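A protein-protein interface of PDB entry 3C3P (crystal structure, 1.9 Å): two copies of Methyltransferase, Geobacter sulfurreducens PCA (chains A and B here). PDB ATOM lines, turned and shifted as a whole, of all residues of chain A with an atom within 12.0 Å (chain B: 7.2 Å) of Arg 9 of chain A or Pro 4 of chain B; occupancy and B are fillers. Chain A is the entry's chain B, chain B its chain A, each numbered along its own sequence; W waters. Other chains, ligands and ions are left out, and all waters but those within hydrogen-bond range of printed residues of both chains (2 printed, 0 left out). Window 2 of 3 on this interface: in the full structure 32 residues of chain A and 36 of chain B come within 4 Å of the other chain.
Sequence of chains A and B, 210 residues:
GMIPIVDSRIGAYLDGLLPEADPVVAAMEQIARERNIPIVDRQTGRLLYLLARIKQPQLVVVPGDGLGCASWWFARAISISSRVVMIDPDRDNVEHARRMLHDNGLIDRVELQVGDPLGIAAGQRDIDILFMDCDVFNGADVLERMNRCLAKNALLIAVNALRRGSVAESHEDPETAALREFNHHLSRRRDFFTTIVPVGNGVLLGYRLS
The backbone carbonyl oxygen (O) of Ile 5 of chain B lies within hydrogen-bond range of the backbone NH (N) of Asp 7 of chain A, at 2.7 Å.
The backbone NH (N) of Asp 7 of chain B is in hydrogen-bond range of the backbone carbonyl oxygen (O) of Ile 5 of chain A, at 2.9 Å.
O of Pro 4 of chain A lies close to OD2 of Asp 7 of chain B (3.2 Å).
OD1 of Asp 7 of chain B is in hydrogen-bond range of OG of Ser 8 of chain B.
The guanidinium group of Arg 9 of chain A lies within salt-bridge range of the side-chain carboxylate of Asp 7 of chain A.
Among the printed residues, pairs that only touch across the chains: Ile 5 of chain A with Val 6 of chain B (3.4 Å), Val 6 of chain A with Ile 5 of chain B (3.2 Å), Asp 7 of chain A with Pro 4 of chain B (3.4 Å), Arg 9 of chain A with Pro 4 of chain B (3.5 Å), Ile 10 of chain A with Pro 4 of chain B (3.6 Å), Ile 10 of chain A with Ala 178 of chain B (3.2 Å), Tyr 13 of chain A with Ala 178 of chain B (3.3 Å) and Pro 198 of chain A with Val 6 of chain B (3.6 Å).
Of the printed residues of chain B, Pro 4 of chain A touches Asp 7 (3.1 Å).
Of chain B, only Pro 4 (3.5 Å) comes within 4 Å of Arg 9 of chain A.
Ala 12 of chain A touches none of the printed residues of chain B.
Leu 14 of chain A touches none of the printed residues of chain B.
No residue of chain A comes within 4 Å of Met 2 of chain B.
Pro 4 of chain B touches just these residues of chain A: Asp 7 (3.4 Å), Arg 9 (3.5 Å) and Ile 10 (3.6 Å).
Of the printed residues of chain A, Ile 5 of chain B touches Val 6 and Asp 7.
Of the printed residues of chain A, Asp 7 of chain B touches Pro 4 (3.1 Å) and Ile 5 (2.9 Å).
Of chain A, only Ile 10 (3.2 Å) and Tyr 13 (3.3 Å) come within 4 Å of Ala 178 of chain B.
The nearest residue of chain B that does not touch Arg 9 of chain A is Ala 178 of chain B (5.5 Å).
The nearest residue of chain A that does not touch Pro 4 of chain B is Val 6 of chain A (6.2 Å).
Hydrophobic or aromatic side chains of chain A within 4 Å of the printed part of chain B: Val 6, Ile 10, Tyr 13 and Pro 198.
Hydrophobic or aromatic side chains of chain B within 4 Å of the printed part of chain A: Pro 4, Val 6 and Ala 178.
Among the printed residues, no Asp or Glu carboxylate lies within 4 Å of a Lys or Arg side-chain nitrogen of the other chain.
Pro 4 of chain A touches Asp 7 of chain B, and with the chains exchanged Asp 7 of chain A touches Pro 4 of chain B.
Ile 5 of chain A touches Val 6 of chain B, and with the chains exchanged Val 6 of chain A touches Ile 5 of chain B.
Ile 5 of chain A touches Asp 7 of chain B, and with the chains exchanged Asp 7 of chain A touches Ile 5 of chain B.
5 positions are printed for both chains.
Of the 11 pairs that touch across the chains among the printed residues, 6 have their exchanged pair printed and touching as well.
Water W2 bridges OD2 of Asp 7 of chain B and O of Pro 4 of chain A.
Water W1 bridges OD2 of Asp 7 of chain A and O of Pro 4 of chain B.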
ATOM      1  N   PRO A   4       1.824  32.089 -24.254  1.00  0.00           N
ATOM      2  CA  PRO A   4       2.655  31.964 -23.048  1.00  0.00           C
ATOM      3  C   PRO A   4       3.696  33.046 -22.945  1.00  0.00           C
ATOM      4  O   PRO A   4       4.297  33.463 -23.941  1.00  0.00           O
ATOM      5  CB  PRO A   4       3.342  30.609 -23.235  1.00  0.00           C
ATOM      6  CG  PRO A   4       3.275  30.343 -24.700  1.00  0.00           C
ATOM      7  CD  PRO A   4       1.983  30.932 -25.152  1.00  0.00           C
ATOM      8  N   ILE A   5       3.856  33.551 -21.743  1.00  0.00           N
ATOM      9  CA  ILE A   5       4.866  34.584 -21.517  1.00  0.00           C
ATOM     10  C   ILE A   5       6.139  33.847 -21.086  1.00  0.00           C
ATOM     11  O   ILE A   5       7.225  34.068 -21.638  1.00  0.00           O
ATOM     12  CB  ILE A   5       4.328  35.673 -20.610  1.00  0.00           C
ATOM     13  CG1 ILE A   5       3.384  36.531 -21.463  1.00  0.00           C
ATOM     14  CG2 ILE A   5       5.460  36.523 -20.019  1.00  0.00           C
ATOM     15  CD1 ILE A   5       2.429  37.407 -20.655  1.00  0.00           C
ATOM     16  N   VAL A   6       5.981  32.966 -20.107  1.00  0.00           N
ATOM     17  CA  VAL A   6       7.092  32.123 -19.650  1.00  0.00           C
ATOM     18  C   VAL A   6       6.620  30.679 -19.673  1.00  0.00           C
ATOM     19  O   VAL A   6       5.457  30.386 -19.491  1.00  0.00           O
ATOM     20  CB  VAL A   6       7.628  32.421 -18.225  1.00  0.00           C
ATOM     21  CG1 VAL A   6       7.901  33.933 -18.024  1.00  0.00           C
ATOM     22  CG2 VAL A   6       6.689  31.900 -17.167  1.00  0.00           C
ATOM     23  N   ASP A   7       7.540  29.803 -19.990  1.00  0.00           N
ATOM     24  CA  ASP A   7       7.282  28.360 -20.010  1.00  0.00           C
ATOM     25  C   ASP A   7       6.409  27.955 -18.801  1.00  0.00           C
ATOM     26  O   ASP A   7       6.696  28.335 -17.672  1.00  0.00           O
ATOM     27  CB  ASP A   7       8.615  27.618 -19.953  1.00  0.00           C
ATOM     28  CG  ASP A   7       8.469  26.137 -20.169  1.00  0.00           C
ATOM     29  OD1 ASP A   7       8.333  25.719 -21.328  1.00  0.00           O
ATOM     30  OD2 ASP A   7       8.597  25.375 -19.200  1.00  0.00           O
ATOM     31  N   SER A   8       5.360  27.161 -19.048  1.00  0.00           N
ATOM     32  CA  SER A   8       4.430  26.748 -17.969  1.00  0.00           C
ATOM     33  C   SER A   8       5.116  25.928 -16.869  1.00  0.00           C
ATOM     34  O   SER A   8       4.672  25.904 -15.711  1.00  0.00           O
ATOM     35  CB  SER A   8       3.219  26.008 -18.544  1.00  0.00           C
ATOM     36  OG  SER A   8       3.616  24.808 -19.164  1.00  0.00           O
ATOM     37  N   ARG A   9       6.215  25.279 -17.215  1.00  0.00           N
ATOM     38  CA  ARG A   9       6.959  24.497 -16.223  1.00  0.00           C
ATOM     39  C   ARG A   9       7.697  25.445 -15.265  1.00  0.00           C
ATOM     40  O   ARG A   9       7.832  25.169 -14.067  1.00  0.00           O
ATOM     41  CB  ARG A   9       7.920  23.525 -16.880  1.00  0.00           C
ATOM     42  CG  ARG A   9       7.202  22.414 -17.596  1.00  0.00           C
ATOM     43  CD  ARG A   9       8.103  21.742 -18.567  1.00  0.00           C
ATOM     44  NE  ARG A   9       8.515  22.680 -19.613  1.00  0.00           N
ATOM     45  CZ  ARG A   9       9.173  22.305 -20.703  1.00  0.00           C
ATOM     46  NH1 ARG A   9       9.450  21.025 -20.872  1.00  0.00           N
ATOM     47  NH2 ARG A   9       9.524  23.185 -21.638  1.00  0.00           N
ATOM     48  N   ILE A  10       8.189  26.553 -15.789  1.00  0.00           N
ATOM     49  CA  ILE A  10       8.879  27.550 -14.959  1.00  0.00           C
ATOM     50  C   ILE A  10       7.869  28.167 -14.012  1.00  0.00           C
ATOM     51  O   ILE A  10       8.117  28.324 -12.821  1.00  0.00           O
ATOM     52  CB  ILE A  10       9.561  28.658 -15.801  1.00  0.00           C
ATOM     53  CG1 ILE A  10      10.698  28.047 -16.611  1.00  0.00           C
ATOM     54  CG2 ILE A  10      10.100  29.779 -14.917  1.00  0.00           C
ATOM     55  CD1 ILE A  10      11.798  27.476 -15.787  1.00  0.00           C
ATOM     56  N   GLY A  11       6.707  28.506 -14.547  1.00  0.00           N
ATOM     57  CA  GLY A  11       5.647  29.149 -13.719  1.00  0.00           C
ATOM     58  C   GLY A  11       5.162  28.273 -12.573  1.00  0.00           C
ATOM     59  O   GLY A  11       4.919  28.754 -11.443  1.00  0.00           O
ATOM     60  N   ALA A  12       5.046  26.987 -12.867  1.00  0.00           N
ATOM     61  CA  ALA A  12       4.607  25.948 -11.910  1.00  0.00           C
ATOM     62  C   ALA A  12       5.638  25.780 -10.790  1.00  0.00           C
ATOM     63  O   ALA A  12       5.320  25.690  -9.604  1.00  0.00           O
ATOM     64  CB  ALA A  12       4.368  24.620 -12.629  1.00  0.00           C
ATOM     65  N   TYR A  13       6.882  25.825 -11.208  1.00  0.00           N
ATOM     66  CA  TYR A  13       8.023  25.714 -10.289  1.00  0.00           C
ATOM     67  C   TYR A  13       8.066  26.921  -9.345  1.00  0.00           C
ATOM     68  O   TYR A  13       8.199  26.769  -8.134  1.00  0.00           O
ATOM     69  CB  TYR A  13       9.351  25.522 -11.076  1.00  0.00           C
ATOM     70  CG  TYR A  13      10.558  25.595 -10.183  1.00  0.00           C
ATOM     71  CD1 TYR A  13      10.873  24.557  -9.314  1.00  0.00           C
ATOM     72  CD2 TYR A  13      11.365  26.713 -10.202  1.00  0.00           C
ATOM     73  CE1 TYR A  13      11.970  24.639  -8.483  1.00  0.00           C
ATOM     74  CE2 TYR A  13      12.463  26.800  -9.403  1.00  0.00           C
ATOM     75  CZ  TYR A  13      12.755  25.772  -8.530  1.00  0.00           C
ATOM     76  OH  TYR A  13      13.871  25.904  -7.717  1.00  0.00           O
ATOM     77  N   LEU A  14       7.902  28.111  -9.903  1.00  0.00           N
ATOM     78  CA  LEU A  14       7.941  29.342  -9.103  1.00  0.00           C
ATOM     79  C   LEU A  14       6.800  29.381  -8.093  1.00  0.00           C
ATOM     80  O   LEU A  14       6.954  29.855  -6.965  1.00  0.00           O
ATOM     81  CB  LEU A  14       7.955  30.577  -9.973  1.00  0.00           C
ATOM     82  CG  LEU A  14       9.186  30.756 -10.876  1.00  0.00           C
ATOM     83  CD1 LEU A  14       9.118  32.065 -11.544  1.00  0.00           C
ATOM     84  CD2 LEU A  14      10.435  30.656 -10.005  1.00  0.00           C
ATOM     85  N   ASP A  15       5.658  28.843  -8.494  1.00  0.00           N
ATOM     86  CA  ASP A  15       4.503  28.755  -7.600  1.00  0.00           C
ATOM     87  C   ASP A  15       4.740  27.758  -6.478  1.00  0.00           C
ATOM     88  O   ASP A  15       4.294  27.966  -5.363  1.00  0.00           O
ATOM     89  CB  ASP A  15       3.227  28.365  -8.347  1.00  0.00           C
ATOM     90  CG  ASP A  15       2.680  29.500  -9.191  1.00  0.00           C
ATOM     91  OD1 ASP A  15       3.098  30.675  -8.994  1.00  0.00           O
ATOM     92  OD2 ASP A  15       1.815  29.204 -10.040  1.00  0.00           O
ATOM     93  N   GLY A  16       5.445  26.677  -6.774  1.00  0.00           N
ATOM     94  CA  GLY A  16       5.702  25.657  -5.759  1.00  0.00           C
ATOM     95  C   GLY A  16       6.585  26.183  -4.651  1.00  0.00           C
ATOM     96  O   GLY A  16       6.497  25.776  -3.505  1.00  0.00           O
ATOM     97  N   LEU A  17       7.442  27.120  -5.018  1.00  0.00           N
ATOM     98  CA  LEU A  17       8.383  27.753  -4.054  1.00  0.00           C
ATOM     99  C   LEU A  17       7.721  28.786  -3.118  1.00  0.00           C
ATOM    100  O   LEU A  17       8.309  29.262  -2.131  1.00  0.00           O
ATOM    101  CB  LEU A  17       9.535  28.439  -4.802  1.00  0.00           C
ATOM    102  CG  LEU A  17      10.663  27.683  -5.473  1.00  0.00           C
ATOM    103  CD1 LEU A  17      11.417  28.711  -6.353  1.00  0.00           C
ATOM    104  CD2 LEU A  17      11.539  27.076  -4.406  1.00  0.00           C
ATOM    105  N   LEU A  18       6.497  29.157  -3.452  1.00  0.00           N
ATOM    106  CA  LEU A  18       5.772  30.123  -2.623  1.00  0.00           C
ATOM    107  C   LEU A  18       5.547  29.677  -1.182  1.00  0.00           C
ATOM    108  O   LEU A  18       5.375  28.471  -0.873  1.00  0.00           O
ATOM    109  CB  LEU A  18       4.426  30.485  -3.246  1.00  0.00           C
ATOM    110  CG  LEU A  18       4.545  31.266  -4.538  1.00  0.00           C
ATOM    111  CD1 LEU A  18       3.185  31.366  -5.145  1.00  0.00           C
ATOM    112  CD2 LEU A  18       5.197  32.674  -4.280  1.00  0.00           C
ATOM    113  N   GLN A  43       2.483  36.380  -7.822  1.00  0.00           N
ATOM    114  CA  GLN A  43       3.895  36.641  -8.155  1.00  0.00           C
ATOM    115  C   GLN A  43       4.095  38.134  -8.414  1.00  0.00           C
ATOM    116  O   GLN A  43       5.109  38.709  -8.057  1.00  0.00           O
ATOM    117  CB  GLN A  43       4.363  35.813  -9.369  1.00  0.00           C
ATOM    118  CG  GLN A  43       4.347  34.272  -9.118  1.00  0.00           C
ATOM    119  CD  GLN A  43       5.402  33.755  -8.098  1.00  0.00           C
ATOM    120  OE1 GLN A  43       6.199  34.517  -7.539  1.00  0.00           O
ATOM    121  NE2 GLN A  43       5.407  32.454  -7.882  1.00  0.00           N
ATOM    122  N   PRO A 198       9.096  39.728 -17.372  1.00  0.00           N
ATOM    123  CA  PRO A 198       8.101  38.735 -17.652  1.00  0.00           C
ATOM    124  C   PRO A 198       7.604  38.025 -16.422  1.00  0.00           C
ATOM    125  O   PRO A 198       7.838  36.850 -16.241  1.00  0.00           O
ATOM    126  CB  PRO A 198       8.814  37.783 -18.626  1.00  0.00           C
ATOM    127  CG  PRO A 198      10.229  37.896 -18.316  1.00  0.00           C
ATOM    128  CD  PRO A 198      10.462  39.218 -17.591  1.00  0.00           C
ATOM    129  N   GLY B   1      16.198  26.652 -25.870  1.00  0.00           N
ATOM    130  CA  GLY B   1      17.330  25.842 -26.403  1.00  0.00           C
ATOM    131  C   GLY B   1      17.841  24.974 -25.277  1.00  0.00           C
ATOM    132  O   GLY B   1      18.111  23.786 -25.446  1.00  0.00           O
ATOM    133  N   MET B   2      17.989  25.604 -24.121  1.00  0.00           N
ATOM    134  CA  MET B   2      18.426  24.903 -22.930  1.00  0.00           C
ATOM    135  C   MET B   2      17.094  24.664 -22.300  1.00  0.00           C
ATOM    136  O   MET B   2      16.174  24.172 -22.953  1.00  0.00           O
ATOM    137  CB  MET B   2      19.265  25.755 -21.981  1.00  0.00           C
ATOM    138  CG  MET B   2      20.342  26.564 -22.643  1.00  0.00           C
ATOM    139  SD  MET B   2      19.726  28.365 -23.128  1.00  0.00           S
ATOM    140  CE  MET B   2      18.079  27.973 -24.084  1.00  0.00           C
ATOM    141  N   ILE B   3      17.010  25.018 -21.026  1.00  0.00           N
ATOM    142  CA  ILE B   3      15.753  24.968 -20.295  1.00  0.00           C
ATOM    143  C   ILE B   3      15.112  26.233 -20.815  1.00  0.00           C
ATOM    144  O   ILE B   3      15.740  27.273 -20.743  1.00  0.00           O
ATOM    145  CB  ILE B   3      15.916  25.067 -18.761  1.00  0.00           C
ATOM    146  CG1 ILE B   3      16.551  23.784 -18.208  1.00  0.00           C
ATOM    147  CG2 ILE B   3      14.576  25.292 -18.090  1.00  0.00           C
ATOM    148  CD1 ILE B   3      15.745  22.536 -18.504  1.00  0.00           C
ATOM    149  N   PRO B   4      13.917  26.150 -21.430  1.00  0.00           N
ATOM    150  CA  PRO B   4      13.313  27.390 -21.909  1.00  0.00           C
ATOM    151  C   PRO B   4      12.611  28.174 -20.792  1.00  0.00           C
ATOM    152  O   PRO B   4      11.975  27.587 -19.898  1.00  0.00           O
ATOM    153  CB  PRO B   4      12.305  26.909 -22.958  1.00  0.00           C
ATOM    154  CG  PRO B   4      11.956  25.539 -22.564  1.00  0.00           C
ATOM    155  CD  PRO B   4      13.139  24.963 -21.835  1.00  0.00           C
ATOM    156  N   ILE B   5      12.761  29.490 -20.827  1.00  0.00           N
ATOM    157  CA  ILE B   5      12.131  30.325 -19.814  1.00  0.00           C
ATOM    158  C   ILE B   5      11.107  31.236 -20.508  1.00  0.00           C
ATOM    159  O   ILE B   5       9.945  30.893 -20.567  1.00  0.00           O
ATOM    160  CB  ILE B   5      13.176  31.032 -18.971  1.00  0.00           C
ATOM    161  CG1 ILE B   5      14.074  29.949 -18.362  1.00  0.00           C
ATOM    162  CG2 ILE B   5      12.529  31.848 -17.877  1.00  0.00           C
ATOM    163  CD1 ILE B   5      15.193  30.453 -17.463  1.00  0.00           C
ATOM    164  N   VAL B   6      11.532  32.366 -21.056  1.00  0.00           N
ATOM    165  CA  VAL B   6      10.593  33.264 -21.751  1.00  0.00           C
ATOM    166  C   VAL B   6      10.300  32.739 -23.180  1.00  0.00           C
ATOM    167  O   VAL B   6      11.205  32.280 -23.876  1.00  0.00           O
ATOM    168  CB  VAL B   6      11.122  34.746 -21.807  1.00  0.00           C
ATOM    169  CG1 VAL B   6      10.097  35.670 -22.462  1.00  0.00           C
ATOM    170  CG2 VAL B   6      11.493  35.281 -20.386  1.00  0.00           C
ATOM    171  N   ASP B   7       9.022  32.753 -23.553  1.00  0.00           N
ATOM    172  CA  ASP B   7       8.567  32.329 -24.883  1.00  0.00           C
ATOM    173  C   ASP B   7       9.391  33.089 -25.920  1.00  0.00           C
ATOM    174  O   ASP B   7       9.570  34.295 -25.839  1.00  0.00           O
ATOM    175  CB  ASP B   7       7.065  32.585 -25.055  1.00  0.00           C
ATOM    176  CG  ASP B   7       6.586  32.322 -26.457  1.00  0.00           C
ATOM    177  OD1 ASP B   7       7.223  31.542 -27.171  1.00  0.00           O
ATOM    178  OD2 ASP B   7       5.556  32.890 -26.867  1.00  0.00           O
ATOM    179  N   SER B   8       9.903  32.352 -26.894  1.00  0.00           N
ATOM    180  CA  SER B   8      10.726  32.921 -27.966  1.00  0.00           C
ATOM    181  C   SER B   8      10.108  34.148 -28.626  1.00  0.00           C
ATOM    182  O   SER B   8      10.799  35.096 -28.977  1.00  0.00           O
ATOM    183  CB  SER B   8      10.999  31.852 -29.039  1.00  0.00           C
ATOM    184  OG  SER B   8       9.791  31.241 -29.463  1.00  0.00           O
ATOM    185  N   ARG B 163      18.349  28.505 -14.703  1.00  0.00           N
ATOM    186  CA  ARG B 163      19.135  27.682 -15.618  1.00  0.00           C
ATOM    187  C   ARG B 163      20.552  28.205 -15.671  1.00  0.00           C
ATOM    188  O   ARG B 163      20.823  29.370 -15.369  1.00  0.00           O
ATOM    189  CB  ARG B 163      18.533  27.646 -17.009  1.00  0.00           C
ATOM    190  CG  ARG B 163      18.655  28.944 -17.717  1.00  0.00           C
ATOM    191  CD  ARG B 163      17.966  28.891 -19.030  1.00  0.00           C
ATOM    192  NE  ARG B 163      18.077  30.176 -19.717  1.00  0.00           N
ATOM    193  CZ  ARG B 163      17.445  30.469 -20.843  1.00  0.00           C
ATOM    194  NH1 ARG B 163      16.656  29.582 -21.413  1.00  0.00           N
ATOM    195  NH2 ARG B 163      17.594  31.652 -21.403  1.00  0.00           N
ATOM    196  N   ALA B 178      13.192  24.236 -14.696  1.00  0.00           N
ATOM    197  CA  ALA B 178      14.393  24.922 -14.198  1.00  0.00           C
ATOM    198  C   ALA B 178      14.345  25.131 -12.709  1.00  0.00           C
ATOM    199  O   ALA B 178      13.364  24.779 -12.060  1.00  0.00           O
ATOM    200  CB  ALA B 178      14.554  26.249 -14.880  1.00  0.00           C
ATOM    201  N   GLY B 200      16.097  36.459 -18.498  1.00  0.00           N
ATOM    202  CA  GLY B 200      17.326  35.733 -18.838  1.00  0.00           C
ATOM    203  C   GLY B 200      17.313  34.281 -18.349  1.00  0.00           C
ATOM    204  O   GLY B 200      16.446  33.505 -18.687  1.00  0.00           O
HETATM  205  O   HOH W   1      11.238  25.153 -18.778  1.00  0.00           O
HETATM  206  O   HOH W   2       3.440  34.061 -27.057  1.00  0.00           O
